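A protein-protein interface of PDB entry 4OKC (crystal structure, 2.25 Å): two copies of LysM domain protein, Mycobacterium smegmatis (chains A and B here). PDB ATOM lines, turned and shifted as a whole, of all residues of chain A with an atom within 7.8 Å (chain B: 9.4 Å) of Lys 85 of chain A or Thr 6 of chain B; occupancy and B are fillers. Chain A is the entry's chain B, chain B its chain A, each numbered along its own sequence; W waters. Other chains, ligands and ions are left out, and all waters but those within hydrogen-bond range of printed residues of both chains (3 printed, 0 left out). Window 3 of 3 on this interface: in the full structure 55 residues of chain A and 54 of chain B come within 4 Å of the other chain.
Among the printed residues, pairs that only touch across the chains: Val 87 of chain A with Asp 3 of chain B (3.2 Å), Lys 85 of chain A with Leu 5 of chain B (3.2 Å), Val 84 of chain A with Gly 62 of chain B (3.2 Å), Leu 86 of chain A with Thr 4 of chain B (3.3 Å), Val 84 of chain A with Val 58 of chain B (3.5 Å), Leu 96 of chain A with Gly 62 of chain B (3.6 Å), Leu 86 of chain A with Phe 64 of chain B (3.6 Å), Leu 86 of chain A with Asp 3 of chain B (3.7 Å), Val 87 of chain A with Thr 4 of chain B (3.7 Å), Val 84 of chain A with Gln 59 of chain B (3.8 Å), Val 84 of chain A with Thr 6 of chain B (3.8 Å), Lys 85 of chain A with Thr 6 of chain B (3.8 Å), Lys 85 of chain A with Thr 4 of chain B (3.8 Å) and Leu 88 of chain A with Leu 17 of chain B (3.9 Å).
Of the printed residues of chain B, Val 84 of chain A touches Thr 6 (3.8 Å), Ala 7 (3.3 Å), Val 58 (3.5 Å), Gln 59 (3.8 Å) and Gly 62 (3.2 Å).
Lys 85 of chain A touches just these residues of chain B: Thr 4 (3.8 Å), Leu 5 (3.2 Å) and Thr 6 (3.8 Å).
Of the printed residues of chain B, Leu 86 of chain A touches Asp 3 (3.7 Å), Thr 4 (3.3 Å), Leu 5 (2.9 Å) and Phe 64 (3.6 Å).
Of the printed residues of chain B, Val 87 of chain A touches Asp 3 and Thr 4.
Printed residues of chain A within 4 Å of Leu 5 of chain B: Lys 85 and Leu 86.
Of chain A, only Val 84 (3.8 Å) and Lys 85 (3.8 Å) come within 4 Å of Thr 6 of chain B.
Of the printed residues of chain A, Gln 59 of chain B touches Val 84.
The nearest residue of chain B that does not touch Lys 85 of chain A is Val 58 of chain B (4.7 Å).
Water W2 lies within hydrogen-bond range of the backbone carbonyl oxygen of Leu 88 of chain A and the side-chain carboxylate of Asp 3 of chain B.
Water W3 bridges N of Glu 83 of chain A and O of Thr 60 of chain B.
Water W1 bridges the backbone carbonyl oxygen (O) of Asp 61 of chain B (3.3 Å) and the side-chain amino group (NZ) of Lys 82 of chain A (3.3 Å).
Of the 18 printed residues of chain A, 6 touch a printed residue of chain B.
Hydrophobic or aromatic side chains of chain A that line the printed part of chain B: Val 84, Leu 86, Val 87, Leu 88 and Leu 96.
Printed residues of chain B that touch a printed residue of chain A: Asp 3, Thr 4, Leu 5, Thr 6, Ala 7, Leu 17, Val 58, Gln 59, Gly 62 and Phe 64.
Hydrophobic or aromatic side chains of chain B within 4 Å of the printed part of chain A: Val 58 and Phe 64.
Among the printed residues, no Asp or Glu carboxylate lies within 4 Å of a Lys or Arg side-chain nitrogen of the other chain.
N of Ala 103 of chain A sits at hydrogen-bond distance from O of Leu 96 of chain A (2.7 Å).
O of Gln 9 of chain B lies within hydrogen-bond range of N of Val 58 of chain B, at 3.0 Å.
The side-chain amide oxygen (OE1) of Gln 9 of chain B sits at hydrogen-bond distance from the backbone NH (N) of Thr 6 of chain B.
The backbone NH of Val 87 of chain A is in hydrogen-bond range of the backbone carbonyl oxygen of Val 95 of chain A (2.7 Å).
The backbone NH of Tyr 97 of chain A sits at hydrogen-bond distance from the backbone carbonyl oxygen of Lys 85 of chain A, 2.7 Å away.
N of Leu 96 of chain A is in hydrogen-bond range of O of Trp 104 of chain A.
N of Leu 86 of chain A lies within hydrogen-bond range of O of Leu 5 of chain B (2.9 Å).
The backbone carbonyl oxygen of Asp 3 of chain B is in hydrogen-bond range of the backbone NH of Leu 88 of chain A, 2.9 Å away.
The backbone carbonyl oxygen of Val 84 of chain A lies within hydrogen-bond range of the backbone NH of Ala 7 of chain B (3.3 Å).
No position is printed for both chains.
Of the 17 pairs that touch across the chains among the printed residues, none has its exchanged pair printed and touching as well.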
ATOM      1  N   LYS A  82      -6.223 -12.344  32.188  1.00  0.00           N
ATOM      2  CA  LYS A  82      -7.416 -12.757  31.437  1.00  0.00           C
ATOM      3  C   LYS A  82      -7.679 -11.908  30.199  1.00  0.00           C
ATOM      4  O   LYS A  82      -7.390 -10.716  30.166  1.00  0.00           O
ATOM      5  CB  LYS A  82      -8.658 -12.757  32.345  1.00  0.00           C
ATOM      6  CG  LYS A  82      -8.408 -13.388  33.701  1.00  0.00           C
ATOM      7  CD  LYS A  82      -9.648 -13.983  34.317  1.00  0.00           C
ATOM      8  CE  LYS A  82      -9.976 -15.318  33.660  1.00  0.00           C
ATOM      9  NZ  LYS A  82      -9.193 -16.448  34.250  1.00  0.00           N
ATOM     10  N   GLU A  83      -8.251 -12.527  29.182  1.00  0.00           N
ATOM     11  CA  GLU A  83      -8.480 -11.842  27.949  1.00  0.00           C
ATOM     12  C   GLU A  83      -7.187 -11.188  27.368  1.00  0.00           C
ATOM     13  O   GLU A  83      -7.212 -10.057  26.881  1.00  0.00           O
ATOM     14  CB  GLU A  83      -9.624 -10.843  28.129  1.00  0.00           C
ATOM     15  CG  GLU A  83     -10.979 -11.484  28.513  1.00  0.00           C
ATOM     16  CD  GLU A  83     -11.956 -10.459  29.147  1.00  0.00           C
ATOM     17  OE1 GLU A  83     -11.694  -9.250  29.032  1.00  0.00           O
ATOM     18  OE2 GLU A  83     -12.984 -10.842  29.764  1.00  0.00           O
ATOM     19  N   VAL A  84      -6.077 -11.928  27.399  1.00  0.00           N
ATOM     20  CA  VAL A  84      -4.808 -11.492  26.822  1.00  0.00           C
ATOM     21  C   VAL A  84      -4.729 -11.392  25.274  1.00  0.00           C
ATOM     22  O   VAL A  84      -5.396 -12.130  24.518  1.00  0.00           O
ATOM     23  CB  VAL A  84      -3.649 -12.353  27.336  1.00  0.00           C
ATOM     24  CG1 VAL A  84      -3.538 -12.202  28.829  1.00  0.00           C
ATOM     25  CG2 VAL A  84      -3.842 -13.831  26.921  1.00  0.00           C
ATOM     26  N   LYS A  85      -3.906 -10.442  24.822  1.00  0.00           N
ATOM     27  CA  LYS A  85      -3.517 -10.293  23.423  1.00  0.00           C
ATOM     28  C   LYS A  85      -2.135  -9.645  23.334  1.00  0.00           C
ATOM     29  O   LYS A  85      -1.834  -8.700  24.075  1.00  0.00           O
ATOM     30  CB  LYS A  85      -4.568  -9.533  22.621  1.00  0.00           C
ATOM     31  CG  LYS A  85      -4.719  -8.061  22.899  1.00  0.00           C
ATOM     32  CD  LYS A  85      -6.052  -7.634  22.317  1.00  0.00           C
ATOM     33  CE  LYS A  85      -6.422  -6.209  22.656  1.00  0.00           C
ATOM     34  NZ  LYS A  85      -5.557  -5.234  21.966  1.00  0.00           N
ATOM     35  N   LEU A  86      -1.312 -10.189  22.443  1.00  0.00           N
ATOM     36  CA  LEU A  86       0.045  -9.772  22.213  1.00  0.00           C
ATOM     37  C   LEU A  86      -0.051  -8.873  21.051  1.00  0.00           C
ATOM     38  O   LEU A  86      -0.691  -9.230  20.062  1.00  0.00           O
ATOM     39  CB  LEU A  86       0.918 -10.965  21.774  1.00  0.00           C
ATOM     40  CG  LEU A  86       2.445 -10.867  21.688  1.00  0.00           C
ATOM     41  CD1 LEU A  86       3.005 -10.633  23.075  1.00  0.00           C
ATOM     42  CD2 LEU A  86       3.071 -12.132  21.101  1.00  0.00           C
ATOM     43  N   VAL A  87       0.601  -7.720  21.141  1.00  0.00           N
ATOM     44  CA  VAL A  87       0.524  -6.735  20.082  1.00  0.00           C
ATOM     45  C   VAL A  87       1.917  -6.246  19.662  1.00  0.00           C
ATOM     46  O   VAL A  87       2.735  -5.892  20.518  1.00  0.00           O
ATOM     47  CB  VAL A  87      -0.362  -5.571  20.492  1.00  0.00           C
ATOM     48  CG1 VAL A  87      -0.333  -4.473  19.435  1.00  0.00           C
ATOM     49  CG2 VAL A  87      -1.773  -6.021  20.701  1.00  0.00           C
ATOM     50  N   LEU A  88       2.187  -6.271  18.355  1.00  0.00           N
ATOM     51  CA  LEU A  88       3.384  -5.623  17.835  1.00  0.00           C
ATOM     52  C   LEU A  88       3.071  -4.173  17.421  1.00  0.00           C
ATOM     53  O   LEU A  88       2.469  -3.953  16.367  1.00  0.00           O
ATOM     54  CB  LEU A  88       3.975  -6.400  16.663  1.00  0.00           C
ATOM     55  CG  LEU A  88       5.174  -5.732  15.981  1.00  0.00           C
ATOM     56  CD1 LEU A  88       6.332  -5.705  16.953  1.00  0.00           C
ATOM     57  CD2 LEU A  88       5.591  -6.404  14.734  1.00  0.00           C
ATOM     58  N   GLN A  89       3.501  -3.206  18.237  1.00  0.00           N
ATOM     59  CA  GLN A  89       3.054  -1.803  18.119  1.00  0.00           C
ATOM     60  C   GLN A  89       3.946  -1.010  17.213  1.00  0.00           C
ATOM     61  O   GLN A  89       5.115  -1.363  17.039  1.00  0.00           O
ATOM     62  CB  GLN A  89       3.029  -1.116  19.467  1.00  0.00           C
ATOM     63  CG  GLN A  89       2.356  -1.936  20.583  1.00  0.00           C
ATOM     64  CD  GLN A  89       2.238  -1.143  21.853  1.00  0.00           C
ATOM     65  OE1 GLN A  89       3.147  -0.379  22.216  1.00  0.00           O
ATOM     66  NE2 GLN A  89       1.104  -1.304  22.542  1.00  0.00           N
ATOM     67  N   LEU A  94       6.628  -4.485  22.071  1.00  0.00           N
ATOM     68  CA  LEU A  94       5.743  -5.640  21.967  1.00  0.00           C
ATOM     69  C   LEU A  94       5.126  -5.890  23.332  1.00  0.00           C
ATOM     70  O   LEU A  94       5.817  -6.200  24.318  1.00  0.00           O
ATOM     71  CB  LEU A  94       6.518  -6.843  21.450  1.00  0.00           C
ATOM     72  CG  LEU A  94       5.790  -8.196  21.342  1.00  0.00           C
ATOM     73  CD1 LEU A  94       4.730  -8.250  20.257  1.00  0.00           C
ATOM     74  CD2 LEU A  94       6.858  -9.343  21.199  1.00  0.00           C
ATOM     75  N   VAL A  95       3.807  -5.753  23.380  1.00  0.00           N
ATOM     76  CA  VAL A  95       3.111  -5.791  24.656  1.00  0.00           C
ATOM     77  C   VAL A  95       2.016  -6.836  24.684  1.00  0.00           C
ATOM     78  O   VAL A  95       1.321  -7.080  23.685  1.00  0.00           O
ATOM     79  CB  VAL A  95       2.472  -4.425  25.020  1.00  0.00           C
ATOM     80  CG1 VAL A  95       1.692  -4.528  26.333  1.00  0.00           C
ATOM     81  CG2 VAL A  95       3.533  -3.320  25.082  1.00  0.00           C
ATOM     82  N   LEU A  96       1.882  -7.441  25.863  1.00  0.00           N
ATOM     83  CA  LEU A  96       0.850  -8.393  26.130  1.00  0.00           C
ATOM     84  C   LEU A  96      -0.173  -7.649  26.934  1.00  0.00           C
ATOM     85  O   LEU A  96       0.083  -7.249  28.062  1.00  0.00           O
ATOM     86  CB  LEU A  96       1.425  -9.588  26.874  1.00  0.00           C
ATOM     87  CG  LEU A  96       0.439 -10.741  27.159  1.00  0.00           C
ATOM     88  CD1 LEU A  96      -0.044 -11.397  25.866  1.00  0.00           C
ATOM     89  CD2 LEU A  96       1.004 -11.792  28.225  1.00  0.00           C
ATOM     90  N   TYR A  97      -1.341  -7.420  26.349  1.00  0.00           N
ATOM     91  CA  TYR A  97      -2.399  -6.722  27.090  1.00  0.00           C
ATOM     92  C   TYR A  97      -3.300  -7.742  27.740  1.00  0.00           C
ATOM     93  O   TYR A  97      -3.702  -8.699  27.126  1.00  0.00           O
ATOM     94  CB  TYR A  97      -3.229  -5.796  26.179  1.00  0.00           C
ATOM     95  CG  TYR A  97      -2.467  -4.586  25.714  1.00  0.00           C
ATOM     96  CD1 TYR A  97      -2.353  -3.473  26.527  1.00  0.00           C
ATOM     97  CD2 TYR A  97      -1.835  -4.568  24.482  1.00  0.00           C
ATOM     98  CE1 TYR A  97      -1.645  -2.375  26.153  1.00  0.00           C
ATOM     99  CE2 TYR A  97      -1.109  -3.469  24.103  1.00  0.00           C
ATOM    100  CZ  TYR A  97      -1.043  -2.358  24.957  1.00  0.00           C
ATOM    101  OH  TYR A  97      -0.317  -1.263  24.584  1.00  0.00           O
ATOM    102  N   ALA A  98      -3.657  -7.477  28.977  1.00  0.00           N
ATOM    103  CA  ALA A  98      -4.550  -8.310  29.706  1.00  0.00           C
ATOM    104  C   ALA A  98      -5.756  -7.460  30.012  1.00  0.00           C
ATOM    105  O   ALA A  98      -5.735  -6.263  29.784  1.00  0.00           O
ATOM    106  CB  ALA A  98      -3.882  -8.761  30.973  1.00  0.00           C
ATOM    107  N   LYS A  99      -6.802  -8.080  30.543  1.00  0.00           N
ATOM    108  CA  LYS A  99      -8.026  -7.400  30.876  1.00  0.00           C
ATOM    109  C   LYS A  99      -7.703  -6.198  31.762  1.00  0.00           C
ATOM    110  O   LYS A  99      -8.290  -5.105  31.605  1.00  0.00           O
ATOM    111  CB  LYS A  99      -8.971  -8.402  31.582  1.00  0.00           C
ATOM    112  CG  LYS A  99     -10.456  -8.055  31.538  1.00  0.00           C
ATOM    113  CD  LYS A  99     -10.842  -7.108  32.678  1.00  0.00           C
ATOM    114  CE  LYS A  99     -12.339  -6.877  32.797  1.00  0.00           C
ATOM    115  NZ  LYS A  99     -13.020  -8.100  33.344  1.00  0.00           N
ATOM    116  N   GLY A 101      -4.944  -4.425  31.994  1.00  0.00           N
ATOM    117  CA  GLY A 101      -3.962  -3.501  31.454  1.00  0.00           C
ATOM    118  C   GLY A 101      -2.750  -4.293  30.960  1.00  0.00           C
ATOM    119  O   GLY A 101      -2.774  -5.520  30.983  1.00  0.00           O
ATOM    120  N   PRO A 102      -1.700  -3.588  30.501  1.00  0.00           N
ATOM    121  CA  PRO A 102      -0.479  -4.197  30.002  1.00  0.00           C
ATOM    122  C   PRO A 102       0.060  -5.169  31.027  1.00  0.00           C
ATOM    123  O   PRO A 102       0.198  -4.830  32.189  1.00  0.00           O
ATOM    124  CB  PRO A 102       0.484  -2.997  29.836  1.00  0.00           C
ATOM    125  CG  PRO A 102      -0.146  -1.891  30.641  1.00  0.00           C
ATOM    126  CD  PRO A 102      -1.618  -2.123  30.436  1.00  0.00           C
ATOM    127  N   ALA A 103       0.335  -6.390  30.600  1.00  0.00           N
ATOM    128  CA  ALA A 103       0.834  -7.389  31.538  1.00  0.00           C
ATOM    129  C   ALA A 103       2.345  -7.551  31.407  1.00  0.00           C
ATOM    130  O   ALA A 103       3.049  -7.806  32.359  1.00  0.00           O
ATOM    131  CB  ALA A 103       0.115  -8.705  31.311  1.00  0.00           C
ATOM    132  N   TRP A 104       2.836  -7.396  30.188  1.00  0.00           N
ATOM    133  CA  TRP A 104       4.186  -7.761  29.869  1.00  0.00           C
ATOM    134  C   TRP A 104       4.541  -6.924  28.656  1.00  0.00           C
ATOM    135  O   TRP A 104       3.675  -6.618  27.855  1.00  0.00           O
ATOM    136  CB  TRP A 104       4.233  -9.266  29.527  1.00  0.00           C
ATOM    137  CG  TRP A 104       5.570  -9.702  29.119  1.00  0.00           C
ATOM    138  CD1 TRP A 104       6.528 -10.279  29.914  1.00  0.00           C
ATOM    139  CD2 TRP A 104       6.161  -9.550  27.815  1.00  0.00           C
ATOM    140  NE1 TRP A 104       7.689 -10.487  29.171  1.00  0.00           N
ATOM    141  CE2 TRP A 104       7.485 -10.050  27.888  1.00  0.00           C
ATOM    142  CE3 TRP A 104       5.696  -9.052  26.591  1.00  0.00           C
ATOM    143  CZ2 TRP A 104       8.341 -10.083  26.769  1.00  0.00           C
ATOM    144  CZ3 TRP A 104       6.550  -9.077  25.503  1.00  0.00           C
ATOM    145  CH2 TRP A 104       7.858  -9.572  25.603  1.00  0.00           C
ATOM    146  N   MET B   1       0.208 -12.659   9.710  1.00  0.00           N
ATOM    147  CA  MET B   1      -0.848 -12.699  10.816  1.00  0.00           C
ATOM    148  C   MET B   1      -1.384 -11.376  11.391  1.00  0.00           C
ATOM    149  O   MET B   1      -2.375 -11.395  12.141  1.00  0.00           O
ATOM    150  CB  MET B   1      -0.486 -13.670  11.966  1.00  0.00           C
ATOM    151  CG  MET B   1      -1.361 -14.921  12.027  1.00  0.00           C
ATOM    152  SD  MET B   1      -0.830 -16.327  13.102  1.00  0.00           S
ATOM    153  CE  MET B   1      -2.354 -16.569  13.953  1.00  0.00           C
ATOM    154  N   ASP B   3      -0.994  -7.578  13.489  1.00  0.00           N
ATOM    155  CA  ASP B   3      -0.156  -7.140  14.630  1.00  0.00           C
ATOM    156  C   ASP B   3      -0.650  -7.683  15.969  1.00  0.00           C
ATOM    157  O   ASP B   3      -0.200  -7.227  17.037  1.00  0.00           O
ATOM    158  CB  ASP B   3      -0.067  -5.616  14.658  1.00  0.00           C
ATOM    159  CG  ASP B   3      -1.382  -4.987  14.977  1.00  0.00           C
ATOM    160  OD1 ASP B   3      -2.402  -5.712  14.958  1.00  0.00           O
ATOM    161  OD2 ASP B   3      -1.385  -3.782  15.268  1.00  0.00           O
ATOM    162  N   THR B   4      -1.587  -8.633  15.928  1.00  0.00           N
ATOM    163  CA  THR B   4      -2.162  -9.093  17.165  1.00  0.00           C
ATOM    164  C   THR B   4      -2.315 -10.645  17.233  1.00  0.00           C
ATOM    165  O   THR B   4      -2.611 -11.289  16.254  1.00  0.00           O
ATOM    166  CB  THR B   4      -3.503  -8.314  17.526  1.00  0.00           C
ATOM    167  OG1 THR B   4      -3.294  -6.898  17.452  1.00  0.00           O
ATOM    168  CG2 THR B   4      -3.943  -8.622  18.945  1.00  0.00           C
ATOM    169  N   LEU B   5      -2.006 -11.206  18.398  1.00  0.00           N
ATOM    170  CA  LEU B   5      -2.252 -12.627  18.719  1.00  0.00           C
ATOM    171  C   LEU B   5      -3.096 -12.713  19.954  1.00  0.00           C
ATOM    172  O   LEU B   5      -2.664 -12.296  21.031  1.00  0.00           O
ATOM    173  CB  LEU B   5      -0.950 -13.393  18.996  1.00  0.00           C
ATOM    174  CG  LEU B   5      -0.410 -14.323  17.909  1.00  0.00           C
ATOM    175  CD1 LEU B   5       0.784 -15.109  18.429  1.00  0.00           C
ATOM    176  CD2 LEU B   5      -1.470 -15.266  17.447  1.00  0.00           C
ATOM    177  N   THR B   6      -4.285 -13.273  19.808  1.00  0.00           N
ATOM    178  CA  THR B   6      -5.198 -13.384  20.939  1.00  0.00           C
ATOM    179  C   THR B   6      -5.142 -14.764  21.591  1.00  0.00           C
ATOM    180  O   THR B   6      -4.487 -15.678  21.053  1.00  0.00           O
ATOM    181  CB  THR B   6      -6.654 -12.975  20.528  1.00  0.00           C
ATOM    182  OG1 THR B   6      -7.083 -13.782  19.418  1.00  0.00           O
ATOM    183  CG2 THR B   6      -6.696 -11.528  20.141  1.00  0.00           C
ATOM    184  N   ALA B   7      -5.810 -14.905  22.751  1.00  0.00           N
ATOM    185  CA  ALA B   7      -5.718 -16.134  23.604  1.00  0.00           C
ATOM    186  C   ALA B   7      -5.994 -17.381  22.788  1.00  0.00           C
ATOM    187  O   ALA B   7      -6.955 -17.415  22.019  1.00  0.00           O
ATOM    188  CB  ALA B   7      -6.702 -16.047  24.853  1.00  0.00           C
ATOM    189  N   GLY B   8      -5.128 -18.379  22.905  1.00  0.00           N
ATOM    190  CA  GLY B   8      -5.198 -19.575  22.074  1.00  0.00           C
ATOM    191  C   GLY B   8      -4.787 -19.408  20.602  1.00  0.00           C
ATOM    192  O   GLY B   8      -4.905 -20.342  19.810  1.00  0.00           O
ATOM    193  N   GLN B   9      -4.301 -18.253  20.184  1.00  0.00           N
ATOM    194  CA  GLN B   9      -3.716 -18.217  18.847  1.00  0.00           C
ATOM    195  C   GLN B   9      -2.227 -18.417  18.977  1.00  0.00           C
ATOM    196  O   GLN B   9      -1.670 -18.175  20.057  1.00  0.00           O
ATOM    197  CB  GLN B   9      -3.990 -16.883  18.166  1.00  0.00           C
ATOM    198  CG  GLN B   9      -5.451 -16.672  17.878  1.00  0.00           C
ATOM    199  CD  GLN B   9      -5.693 -15.334  17.207  1.00  0.00           C
ATOM    200  OE1 GLN B   9      -4.837 -14.434  17.265  1.00  0.00           O
ATOM    201  NE2 GLN B   9      -6.870 -15.193  16.571  1.00  0.00           N
ATOM    202  N   LYS B  10      -1.580 -18.836  17.897  1.00  0.00           N
ATOM    203  CA  LYS B  10      -0.149 -19.104  17.931  1.00  0.00           C
ATOM    204  C   LYS B  10       0.573 -18.826  16.629  1.00  0.00           C
ATOM    205  O   LYS B  10      -0.004 -18.867  15.554  1.00  0.00           O
ATOM    206  CB  LYS B  10       0.118 -20.570  18.361  1.00  0.00           C
ATOM    207  CG  LYS B  10      -0.288 -21.535  17.313  1.00  0.00           C
ATOM    208  CD  LYS B  10      -0.574 -22.903  17.882  1.00  0.00           C
ATOM    209  CE  LYS B  10      -1.403 -23.667  16.859  1.00  0.00           C
ATOM    210  NZ  LYS B  10      -1.086 -23.157  15.469  1.00  0.00           N
ATOM    211  N   LEU B  11       1.859 -18.543  16.761  1.00  0.00           N
ATOM    212  CA  LEU B  11       2.744 -18.423  15.616  1.00  0.00           C
ATOM    213  C   LEU B  11       3.518 -19.745  15.445  1.00  0.00           C
ATOM    214  O   LEU B  11       4.026 -20.330  16.415  1.00  0.00           O
ATOM    215  CB  LEU B  11       3.775 -17.336  15.836  1.00  0.00           C
ATOM    216  CG  LEU B  11       3.426 -15.886  15.697  1.00  0.00           C
ATOM    217  CD1 LEU B  11       4.626 -15.128  16.319  1.00  0.00           C
ATOM    218  CD2 LEU B  11       3.216 -15.656  14.213  1.00  0.00           C
ATOM    219  N   LEU B  17       4.025 -11.717  13.057  1.00  0.00           N
ATOM    220  CA  LEU B  17       3.270 -10.500  13.263  1.00  0.00           C
ATOM    221  C   LEU B  17       4.042  -9.406  12.594  1.00  0.00           C
ATOM    222  O   LEU B  17       5.255  -9.523  12.404  1.00  0.00           O
ATOM    223  CB  LEU B  17       3.176 -10.162  14.759  1.00  0.00           C
ATOM    224  CG  LEU B  17       2.351 -11.046  15.723  1.00  0.00           C
ATOM    225  CD1 LEU B  17       2.428 -10.475  17.144  1.00  0.00           C
ATOM    226  CD2 LEU B  17       0.866 -11.183  15.248  1.00  0.00           C
ATOM    227  N   ALA B  56       4.844 -20.456  19.214  1.00  0.00           N
ATOM    228  CA  ALA B  56       4.887 -19.390  20.155  1.00  0.00           C
ATOM    229  C   ALA B  56       3.417 -19.036  20.286  1.00  0.00           C
ATOM    230  O   ALA B  56       2.801 -18.517  19.345  1.00  0.00           O
ATOM    231  CB  ALA B  56       5.690 -18.221  19.575  1.00  0.00           C
ATOM    232  N   GLU B  57       2.847 -19.362  21.440  1.00  0.00           N
ATOM    233  CA  GLU B  57       1.425 -19.294  21.593  1.00  0.00           C
ATOM    234  C   GLU B  57       0.953 -18.457  22.758  1.00  0.00           C
ATOM    235  O   GLU B  57       1.457 -18.599  23.902  1.00  0.00           O
ATOM    236  CB  GLU B  57       0.858 -20.697  21.681  1.00  0.00           C
ATOM    237  CG  GLU B  57      -0.523 -20.782  22.344  1.00  0.00           C
ATOM    238  CD  GLU B  57      -1.321 -21.999  21.898  1.00  0.00           C
ATOM    239  OE1 GLU B  57      -0.679 -23.041  21.562  1.00  0.00           O
ATOM    240  OE2 GLU B  57      -2.586 -21.899  21.893  1.00  0.00           O
ATOM    241  N   VAL B  58      -0.022 -17.579  22.464  1.00  0.00           N
ATOM    242  CA  VAL B  58      -0.652 -16.811  23.505  1.00  0.00           C
ATOM    243  C   VAL B  58      -1.659 -17.798  24.018  1.00  0.00           C
ATOM    244  O   VAL B  58      -2.618 -18.120  23.314  1.00  0.00           O
ATOM    245  CB  VAL B  58      -1.375 -15.522  22.998  1.00  0.00           C
ATOM    246  CG1 VAL B  58      -1.838 -14.658  24.198  1.00  0.00           C
ATOM    247  CG2 VAL B  58      -0.499 -14.716  22.053  1.00  0.00           C
ATOM    248  N   GLN B  59      -1.396 -18.297  25.230  1.00  0.00           N
ATOM    249  CA  GLN B  59      -2.217 -19.328  25.897  1.00  0.00           C
ATOM    250  C   GLN B  59      -3.516 -18.781  26.450  1.00  0.00           C
ATOM    251  O   GLN B  59      -3.701 -17.591  26.527  1.00  0.00           O
ATOM    252  CB  GLN B  59      -1.411 -20.040  26.980  1.00  0.00           C
ATOM    253  CG  GLN B  59      -0.539 -21.194  26.450  1.00  0.00           C
ATOM    254  CD  GLN B  59       0.428 -21.749  27.515  1.00  0.00           C
ATOM    255  OE1 GLN B  59       0.107 -21.831  28.698  1.00  0.00           O
ATOM    256  NE2 GLN B  59       1.618 -22.128  27.080  1.00  0.00           N
ATOM    257  N   THR B  60      -4.441 -19.654  26.797  1.00  0.00           N
ATOM    258  CA  THR B  60      -5.750 -19.199  27.247  1.00  0.00           C
ATOM    259  C   THR B  60      -5.790 -18.941  28.777  1.00  0.00           C
ATOM    260  O   THR B  60      -6.803 -18.542  29.323  1.00  0.00           O
ATOM    261  CB  THR B  60      -6.858 -20.209  26.811  1.00  0.00           C
ATOM    262  OG1 THR B  60      -8.124 -19.751  27.277  1.00  0.00           O
ATOM    263  CG2 THR B  60      -6.587 -21.606  27.377  1.00  0.00           C
ATOM    264  N   ASP B  61      -4.679 -19.208  29.452  1.00  0.00           N
ATOM    265  CA  ASP B  61      -4.496 -18.840  30.848  1.00  0.00           C
ATOM    266  C   ASP B  61      -3.730 -17.516  30.848  1.00  0.00           C
ATOM    267  O   ASP B  61      -3.168 -17.122  31.859  1.00  0.00           O
ATOM    268  CB  ASP B  61      -3.726 -19.927  31.628  1.00  0.00           C
ATOM    269  CG  ASP B  61      -2.270 -20.115  31.135  1.00  0.00           C
ATOM    270  OD1 ASP B  61      -1.485 -19.138  31.017  1.00  0.00           O
ATOM    271  OD2 ASP B  61      -1.895 -21.259  30.878  1.00  0.00           O
ATOM    272  N   GLY B  62      -3.685 -16.867  29.683  1.00  0.00           N
ATOM    273  CA  GLY B  62      -3.072 -15.549  29.562  1.00  0.00           C
ATOM    274  C   GLY B  62      -1.550 -15.558  29.434  1.00  0.00           C
ATOM    275  O   GLY B  62      -0.946 -14.507  29.440  1.00  0.00           O
ATOM    276  N   ASN B  63      -0.929 -16.744  29.354  1.00  0.00           N
ATOM    277  CA  ASN B  63       0.539 -16.859  29.223  1.00  0.00           C
ATOM    278  C   ASN B  63       0.958 -17.059  27.750  1.00  0.00           C
ATOM    279  O   ASN B  63       0.363 -17.846  27.035  1.00  0.00           O
ATOM    280  CB  ASN B  63       1.093 -17.993  30.130  1.00  0.00           C
ATOM    281  CG  ASN B  63       2.607 -17.856  30.435  1.00  0.00           C
ATOM    282  OD1 ASN B  63       3.266 -16.893  30.054  1.00  0.00           O
ATOM    283  ND2 ASN B  63       3.148 -18.839  31.117  1.00  0.00           N
ATOM    284  N   PHE B  64       1.976 -16.331  27.310  1.00  0.00           N
ATOM    285  CA  PHE B  64       2.535 -16.498  25.961  1.00  0.00           C
ATOM    286  C   PHE B  64       3.767 -17.385  26.094  1.00  0.00           C
ATOM    287  O   PHE B  64       4.611 -17.147  26.948  1.00  0.00           O
ATOM    288  CB  PHE B  64       2.891 -15.126  25.375  1.00  0.00           C
ATOM    289  CG  PHE B  64       3.611 -15.185  24.052  1.00  0.00           C
ATOM    290  CD1 PHE B  64       3.125 -15.992  23.018  1.00  0.00           C
ATOM    291  CD2 PHE B  64       4.735 -14.384  23.812  1.00  0.00           C
ATOM    292  CE1 PHE B  64       3.774 -16.077  21.788  1.00  0.00           C
ATOM    293  CE2 PHE B  64       5.393 -14.433  22.538  1.00  0.00           C
ATOM    294  CZ  PHE B  64       4.898 -15.308  21.540  1.00  0.00           C
HETATM  295  O   HOH W   1      -6.004 -16.344  33.320  1.00  0.00           O
HETATM  296  O   HOH W   2       1.090  -2.207  15.088  1.00  0.00           O
HETATM  297  O   HOH W   3      -7.193 -15.199  28.487  1.00  0.00           O
